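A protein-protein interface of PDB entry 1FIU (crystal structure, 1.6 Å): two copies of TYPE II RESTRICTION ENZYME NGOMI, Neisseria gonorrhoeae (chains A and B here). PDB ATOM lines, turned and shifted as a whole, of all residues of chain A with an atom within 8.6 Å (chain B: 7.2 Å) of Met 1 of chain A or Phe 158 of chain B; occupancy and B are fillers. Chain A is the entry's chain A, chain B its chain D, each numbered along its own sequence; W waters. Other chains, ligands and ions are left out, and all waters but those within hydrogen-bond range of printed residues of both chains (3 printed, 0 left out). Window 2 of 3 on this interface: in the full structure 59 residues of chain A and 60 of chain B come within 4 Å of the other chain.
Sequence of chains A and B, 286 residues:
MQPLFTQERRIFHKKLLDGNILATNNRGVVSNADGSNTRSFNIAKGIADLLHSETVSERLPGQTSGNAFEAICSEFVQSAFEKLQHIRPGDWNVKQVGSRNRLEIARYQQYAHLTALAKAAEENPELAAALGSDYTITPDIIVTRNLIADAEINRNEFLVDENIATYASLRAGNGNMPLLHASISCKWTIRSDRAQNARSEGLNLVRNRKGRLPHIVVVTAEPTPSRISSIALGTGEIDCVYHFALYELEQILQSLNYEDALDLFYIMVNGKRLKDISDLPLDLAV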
ATOM      1  N   MET A   1      23.157  26.348   2.443  1.00  0.00           N
ATOM      2  CA  MET A   1      23.740  25.139   3.105  1.00  0.00           C
ATOM      3  C   MET A   1      22.686  24.549   4.037  1.00  0.00           C
ATOM      4  O   MET A   1      22.485  25.045   5.150  1.00  0.00           O
ATOM      5  CB  MET A   1      24.983  25.532   3.923  1.00  0.00           C
ATOM      6  CG  MET A   1      26.303  24.851   3.527  1.00  0.00           C
ATOM      7  SD  MET A   1      26.514  23.138   4.126  1.00  0.00           S
ATOM      8  CE  MET A   1      27.119  22.304   2.631  1.00  0.00           C
ATOM      9  N   GLN A   2      21.990  23.520   3.573  1.00  0.00           N
ATOM     10  CA  GLN A   2      20.988  22.869   4.405  1.00  0.00           C
ATOM     11  C   GLN A   2      21.768  21.930   5.327  1.00  0.00           C
ATOM     12  O   GLN A   2      22.678  21.242   4.887  1.00  0.00           O
ATOM     13  CB  GLN A   2      20.006  22.069   3.539  1.00  0.00           C
ATOM     14  CG  GLN A   2      18.971  22.923   2.807  1.00  0.00           C
ATOM     15  CD  GLN A   2      18.258  22.160   1.708  1.00  0.00           C
ATOM     16  OE1 GLN A   2      18.223  20.925   1.717  1.00  0.00           O
ATOM     17  NE2 GLN A   2      17.673  22.893   0.755  1.00  0.00           N
ATOM     18  N   PRO A   3      21.453  21.931   6.626  1.00  0.00           N
ATOM     19  CA  PRO A   3      22.182  21.032   7.534  1.00  0.00           C
ATOM     20  C   PRO A   3      21.976  19.572   7.139  1.00  0.00           C
ATOM     21  O   PRO A   3      21.038  19.249   6.417  1.00  0.00           O
ATOM     22  CB  PRO A   3      21.610  21.383   8.907  1.00  0.00           C
ATOM     23  CG  PRO A   3      20.255  21.895   8.604  1.00  0.00           C
ATOM     24  CD  PRO A   3      20.434  22.708   7.341  1.00  0.00           C
ATOM     25  N   LEU A   4      22.846  18.678   7.603  1.00  0.00           N
ATOM     26  CA  LEU A   4      22.724  17.283   7.210  1.00  0.00           C
ATOM     27  C   LEU A   4      21.449  16.573   7.629  1.00  0.00           C
ATOM     28  O   LEU A   4      21.000  15.695   6.911  1.00  0.00           O
ATOM     29  CB  LEU A   4      23.938  16.470   7.671  1.00  0.00           C
ATOM     30  CG  LEU A   4      25.268  16.893   7.053  1.00  0.00           C
ATOM     31  CD1 LEU A   4      26.339  15.882   7.457  1.00  0.00           C
ATOM     32  CD2 LEU A   4      25.152  16.971   5.530  1.00  0.00           C
ATOM     33  N   PHE A   5      20.878  16.925   8.779  1.00  0.00           N
ATOM     34  CA  PHE A   5      19.644  16.259   9.179  1.00  0.00           C
ATOM     35  C   PHE A   5      18.495  16.682   8.261  1.00  0.00           C
ATOM     36  O   PHE A   5      17.554  15.914   8.054  1.00  0.00           O
ATOM     37  CB  PHE A   5      19.329  16.524  10.649  1.00  0.00           C
ATOM     38  CG  PHE A   5      20.109  15.629  11.609  1.00  0.00           C
ATOM     39  CD1 PHE A   5      19.916  15.723  12.980  1.00  0.00           C
ATOM     40  CD2 PHE A   5      21.025  14.697  11.128  1.00  0.00           C
ATOM     41  CE1 PHE A   5      20.634  14.895  13.863  1.00  0.00           C
ATOM     42  CE2 PHE A   5      21.737  13.869  11.994  1.00  0.00           C
ATOM     43  CZ  PHE A   5      21.539  13.970  13.356  1.00  0.00           C
ATOM     44  N   THR A   6      18.588  17.890   7.692  1.00  0.00           N
ATOM     45  CA  THR A   6      17.551  18.344   6.767  1.00  0.00           C
ATOM     46  C   THR A   6      17.732  17.548   5.472  1.00  0.00           C
ATOM     47  O   THR A   6      16.752  17.075   4.873  1.00  0.00           O
ATOM     48  CB  THR A   6      17.671  19.866   6.499  1.00  0.00           C
ATOM     49  OG1 THR A   6      17.507  20.568   7.738  1.00  0.00           O
ATOM     50  CG2 THR A   6      16.592  20.346   5.511  1.00  0.00           C
ATOM     51  N   GLN A   7      18.983  17.359   5.060  1.00  0.00           N
ATOM     52  CA  GLN A   7      19.273  16.594   3.859  1.00  0.00           C
ATOM     53  C   GLN A   7      18.795  15.145   4.028  1.00  0.00           C
ATOM     54  O   GLN A   7      18.205  14.557   3.118  1.00  0.00           O
ATOM     55  CB  GLN A   7      20.773  16.632   3.563  1.00  0.00           C
ATOM     56  CG  GLN A   7      21.268  18.032   3.243  1.00  0.00           C
ATOM     57  CD  GLN A   7      22.712  18.071   2.813  1.00  0.00           C
ATOM     58  OE1 GLN A   7      23.161  17.228   2.030  1.00  0.00           O
ATOM     59  NE2 GLN A   7      23.450  19.063   3.307  1.00  0.00           N
ATOM     60  N   ARG A  10      15.051  14.884   3.719  1.00  0.00           N
ATOM     61  CA  ARG A  10      14.605  14.946   2.324  1.00  0.00           C
ATOM     62  C   ARG A  10      14.856  13.628   1.610  1.00  0.00           C
ATOM     63  O   ARG A  10      14.049  13.183   0.807  1.00  0.00           O
ATOM     64  CB  ARG A  10      15.305  16.112   1.605  1.00  0.00           C
ATOM     65  CG  ARG A  10      14.916  17.434   2.236  1.00  0.00           C
ATOM     66  CD  ARG A  10      15.488  18.670   1.548  1.00  0.00           C
ATOM     67  NE  ARG A  10      15.090  19.878   2.273  1.00  0.00           N
ATOM     68  CZ  ARG A  10      15.235  21.115   1.809  1.00  0.00           C
ATOM     69  NH1 ARG A  10      15.770  21.322   0.611  1.00  0.00           N
ATOM     70  NH2 ARG A  10      14.847  22.151   2.546  1.00  0.00           N
ATOM     71  N   LYS A  83      25.716   9.850  12.739  1.00  0.00           N
ATOM     72  CA  LYS A  83      26.398  11.140  12.844  1.00  0.00           C
ATOM     73  C   LYS A  83      26.448  11.706  14.263  1.00  0.00           C
ATOM     74  O   LYS A  83      27.018  12.773  14.505  1.00  0.00           O
ATOM     75  CB  LYS A  83      25.734  12.155  11.891  1.00  0.00           C
ATOM     76  CG  LYS A  83      25.757  11.666  10.447  1.00  0.00           C
ATOM     77  CD  LYS A  83      25.159  12.654   9.467  1.00  0.00           C
ATOM     78  CE  LYS A  83      25.314  12.134   8.026  1.00  0.00           C
ATOM     79  NZ  LYS A  83      26.764  11.943   7.651  1.00  0.00           N
ATOM     80  N   ILE B 153      26.455  19.742  19.061  1.00  0.00           N
ATOM     81  CA  ILE B 153      25.798  18.807  18.146  1.00  0.00           C
ATOM     82  C   ILE B 153      26.535  18.901  16.800  1.00  0.00           C
ATOM     83  O   ILE B 153      26.846  17.884  16.175  1.00  0.00           O
ATOM     84  CB  ILE B 153      24.281  19.146  17.966  1.00  0.00           C
ATOM     85  CG1 ILE B 153      23.533  18.878  19.285  1.00  0.00           C
ATOM     86  CG2 ILE B 153      23.664  18.332  16.814  1.00  0.00           C
ATOM     87  CD1 ILE B 153      22.068  19.354  19.300  1.00  0.00           C
ATOM     88  N   ASN B 154      26.848  20.133  16.381  1.00  0.00           N
ATOM     89  CA  ASN B 154      27.531  20.379  15.106  1.00  0.00           C
ATOM     90  C   ASN B 154      29.043  20.433  15.265  1.00  0.00           C
ATOM     91  O   ASN B 154      29.731  21.103  14.495  1.00  0.00           O
ATOM     92  CB  ASN B 154      27.082  21.722  14.505  1.00  0.00           C
ATOM     93  CG  ASN B 154      25.606  21.751  14.148  1.00  0.00           C
ATOM     94  OD1 ASN B 154      24.992  20.713  13.900  1.00  0.00           O
ATOM     95  ND2 ASN B 154      25.030  22.951  14.102  1.00  0.00           N
ATOM     96  N   ARG B 155      29.569  19.739  16.263  1.00  0.00           N
ATOM     97  CA  ARG B 155      31.005  19.760  16.498  1.00  0.00           C
ATOM     98  C   ARG B 155      31.823  19.330  15.284  1.00  0.00           C
ATOM     99  O   ARG B 155      32.816  19.974  14.939  1.00  0.00           O
ATOM    100  CB  ARG B 155      31.341  18.865  17.695  1.00  0.00           C
ATOM    101  CG  ARG B 155      32.824  18.677  17.922  1.00  0.00           C
ATOM    102  CD  ARG B 155      33.221  19.075  19.333  1.00  0.00           C
ATOM    103  NE  ARG B 155      32.680  18.184  20.362  1.00  0.00           N
ATOM    104  CZ  ARG B 155      32.933  16.876  20.438  1.00  0.00           C
ATOM    105  NH1 ARG B 155      33.719  16.290  19.539  1.00  0.00           N
ATOM    106  NH2 ARG B 155      32.424  16.157  21.433  1.00  0.00           N
ATOM    107  N   ASN B 156      31.405  18.253  14.624  1.00  0.00           N
ATOM    108  CA  ASN B 156      32.139  17.719  13.477  1.00  0.00           C
ATOM    109  C   ASN B 156      31.524  17.962  12.100  1.00  0.00           C
ATOM    110  O   ASN B 156      32.223  17.958  11.080  1.00  0.00           O
ATOM    111  CB  ASN B 156      32.350  16.211  13.670  1.00  0.00           C
ATOM    112  CG  ASN B 156      33.085  15.892  14.963  1.00  0.00           C
ATOM    113  OD1 ASN B 156      34.049  16.566  15.310  1.00  0.00           O
ATOM    114  ND2 ASN B 156      32.635  14.864  15.675  1.00  0.00           N
ATOM    115  N   GLU B 157      30.219  18.163  12.071  1.00  0.00           N
ATOM    116  CA  GLU B 157      29.509  18.376  10.822  1.00  0.00           C
ATOM    117  C   GLU B 157      28.364  19.322  11.082  1.00  0.00           C
ATOM    118  O   GLU B 157      27.974  19.545  12.226  1.00  0.00           O
ATOM    119  CB  GLU B 157      28.949  17.048  10.290  1.00  0.00           C
ATOM    120  CG  GLU B 157      29.970  15.938  10.142  1.00  0.00           C
ATOM    121  CD  GLU B 157      29.332  14.621   9.732  1.00  0.00           C
ATOM    122  OE1 GLU B 157      29.140  14.391   8.518  1.00  0.00           O
ATOM    123  OE2 GLU B 157      29.000  13.813  10.628  1.00  0.00           O
ATOM    124  N   PHE B 158      27.816  19.889  10.014  1.00  0.00           N
ATOM    125  CA  PHE B 158      26.700  20.811  10.150  1.00  0.00           C
ATOM    126  C   PHE B 158      25.442  19.952  10.121  1.00  0.00           C
ATOM    127  O   PHE B 158      24.862  19.704   9.063  1.00  0.00           O
ATOM    128  CB  PHE B 158      26.709  21.808   8.987  1.00  0.00           C
ATOM    129  CG  PHE B 158      25.624  22.839   9.057  1.00  0.00           C
ATOM    130  CD1 PHE B 158      25.264  23.404  10.271  1.00  0.00           C
ATOM    131  CD2 PHE B 158      24.976  23.266   7.900  1.00  0.00           C
ATOM    132  CE1 PHE B 158      24.275  24.386  10.338  1.00  0.00           C
ATOM    133  CE2 PHE B 158      23.992  24.242   7.959  1.00  0.00           C
ATOM    134  CZ  PHE B 158      23.638  24.803   9.180  1.00  0.00           C
ATOM    135  N   LEU B 159      25.026  19.495  11.299  1.00  0.00           N
ATOM    136  CA  LEU B 159      23.858  18.623  11.411  1.00  0.00           C
ATOM    137  C   LEU B 159      22.505  19.306  11.581  1.00  0.00           C
ATOM    138  O   LEU B 159      21.502  18.862  11.005  1.00  0.00           O
ATOM    139  CB  LEU B 159      24.055  17.663  12.592  1.00  0.00           C
ATOM    140  CG  LEU B 159      25.294  16.777  12.566  1.00  0.00           C
ATOM    141  CD1 LEU B 159      25.263  15.864  13.803  1.00  0.00           C
ATOM    142  CD2 LEU B 159      25.305  15.948  11.308  1.00  0.00           C
ATOM    143  N   VAL B 160      22.449  20.352  12.402  1.00  0.00           N
ATOM    144  CA  VAL B 160      21.182  21.024  12.650  1.00  0.00           C
ATOM    145  C   VAL B 160      21.256  22.545  12.630  1.00  0.00           C
ATOM    146  O   VAL B 160      22.325  23.131  12.802  1.00  0.00           O
ATOM    147  CB  VAL B 160      20.601  20.638  14.045  1.00  0.00           C
ATOM    148  CG1 VAL B 160      20.321  19.136  14.120  1.00  0.00           C
ATOM    149  CG2 VAL B 160      21.579  21.051  15.145  1.00  0.00           C
ATOM    150  N   ASP B 161      20.103  23.163  12.393  1.00  0.00           N
ATOM    151  CA  ASP B 161      19.952  24.612  12.450  1.00  0.00           C
ATOM    152  C   ASP B 161      18.591  24.828  13.142  1.00  0.00           C
ATOM    153  O   ASP B 161      18.023  23.875  13.668  1.00  0.00           O
ATOM    154  CB  ASP B 161      20.061  25.271  11.055  1.00  0.00           C
ATOM    155  CG  ASP B 161      18.870  25.013  10.145  1.00  0.00           C
ATOM    156  OD1 ASP B 161      17.925  24.282  10.509  1.00  0.00           O
ATOM    157  OD2 ASP B 161      18.893  25.572   9.022  1.00  0.00           O
ATOM    158  N   GLU B 162      18.063  26.048  13.177  1.00  0.00           N
ATOM    159  CA  GLU B 162      16.801  26.270  13.877  1.00  0.00           C
ATOM    160  C   GLU B 162      15.543  25.743  13.212  1.00  0.00           C
ATOM    161  O   GLU B 162      14.475  25.822  13.797  1.00  0.00           O
ATOM    162  CB  GLU B 162      16.604  27.759  14.176  1.00  0.00           C
ATOM    163  CG  GLU B 162      16.867  28.668  12.990  1.00  0.00           C
ATOM    164  CD  GLU B 162      18.332  28.648  12.584  1.00  0.00           C
ATOM    165  OE1 GLU B 162      19.193  28.739  13.490  1.00  0.00           O
ATOM    166  OE2 GLU B 162      18.626  28.538  11.372  1.00  0.00           O
HETATM  167  O   HOH W   1      28.737  14.485  13.238  1.00  0.00           O
HETATM  168  O   HOH W   2      16.807  23.100   8.173  1.00  0.00           O
HETATM  169  O   HOH W   3      30.356  12.491  15.222  1.00  0.00           O
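The backbone NH of Leu 159 of chain B lies within hydrogen-bond range of the side-chain amide oxygen of Asn 154 of chain B (2.9 Å).
N of Val 160 of chain B lies within hydrogen-bond range of OD1 of Asn 154 of chain B, 3.0 Å away.
No position is printed for both chains.
Of the 12 pairs that touch across the chains among the printed residues, none has its exchanged pair printed and touching as well.
Met 1 of chain A touches just one residue of chain B: Phe 158.
Printed residues of chain B within 4 Å of Pro 3 of chain A: Phe 158 (3.4 Å), Leu 159 (3.3 Å), Val 160 (3.7 Å) and Asp 161 (3.7 Å).
Of the printed residues of chain B, Leu 4 of chain A touches Glu 157, Phe 158 and Leu 159.
Gln 7 of chain A touches none of the printed residues of chain B.
Printed residues of chain B within 4 Å of Lys 83 of chain A: Glu 157 and Leu 159.
Ile 153 of chain B touches none of the printed residues of chain A.
Of the printed residues of chain A, Glu 157 of chain B touches Leu 4 (3.3 Å) and Lys 83 (3.5 Å).
Of the printed residues of chain A, Asp 161 of chain B touches Pro 3.
The nearest residue of chain A that does not touch Phe 158 of chain B is Gln 2 of chain A (4.1 Å).
The nearest printed residue of chain B that does not touch Leu 4 of chain A is Val 160 of chain B (5.1 Å).
Among the printed residues, pairs that only touch across the chains: Pro 3 of chain A with Leu 159 of chain B (3.3 Å), Met 1 of chain A with Phe 158 of chain B (3.3 Å), Leu 4 of chain A with Glu 157 of chain B (3.3 Å), Pro 3 of chain A with Phe 158 of chain B (3.4 Å), Phe 5 of chain A with Val 160 of chain B (3.6 Å), Lys 83 of chain A with Leu 159 of chain B (3.6 Å), Pro 3 of chain A with Asp 161 of chain B (3.7 Å), Leu 4 of chain A with Leu 159 of chain B (3.7 Å) and Pro 3 of chain A with Val 160 of chain B (3.7 Å).
Of the 9 printed residues of chain A, 5 touch a printed residue of chain B.
Hydrophobic or aromatic side chains of chain B that line the printed part of chain A: Phe 158, Leu 159 and Val 160.
Among the printed residues, Asp or Glu carboxylates within 4 Å of a Lys or Arg side-chain nitrogen of the other chain: Lys 83 of chain A with Glu 157 of chain B (3.5 Å).
N of Leu 4 of chain A lies within hydrogen-bond range of O of Phe 158 of chain B (2.7 Å).
O of Leu 159 of chain B sits at hydrogen-bond distance from N of Phe 5 of chain A (3.0 Å).
NZ of Lys 83 of chain A is in salt-bridge range of OE1 of Glu 157 of chain B, 3.5 Å away.
Water W2 lies within hydrogen-bond range of the side-chain hydroxyl (OG1) of Thr 6 of chain A (2.7 Å) and the side-chain carboxylate (OD1) of Asp 161 of chain B (2.8 Å).
Water W1 bridges OE2 of Glu 157 of chain B and O of Lys 83 of chain A.
Water W3 bridges the side-chain amide nitrogen of Asn 156 of chain B (3.3 Å) and the backbone carbonyl oxygen of Lys 83 of chain A (3.4 Å).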
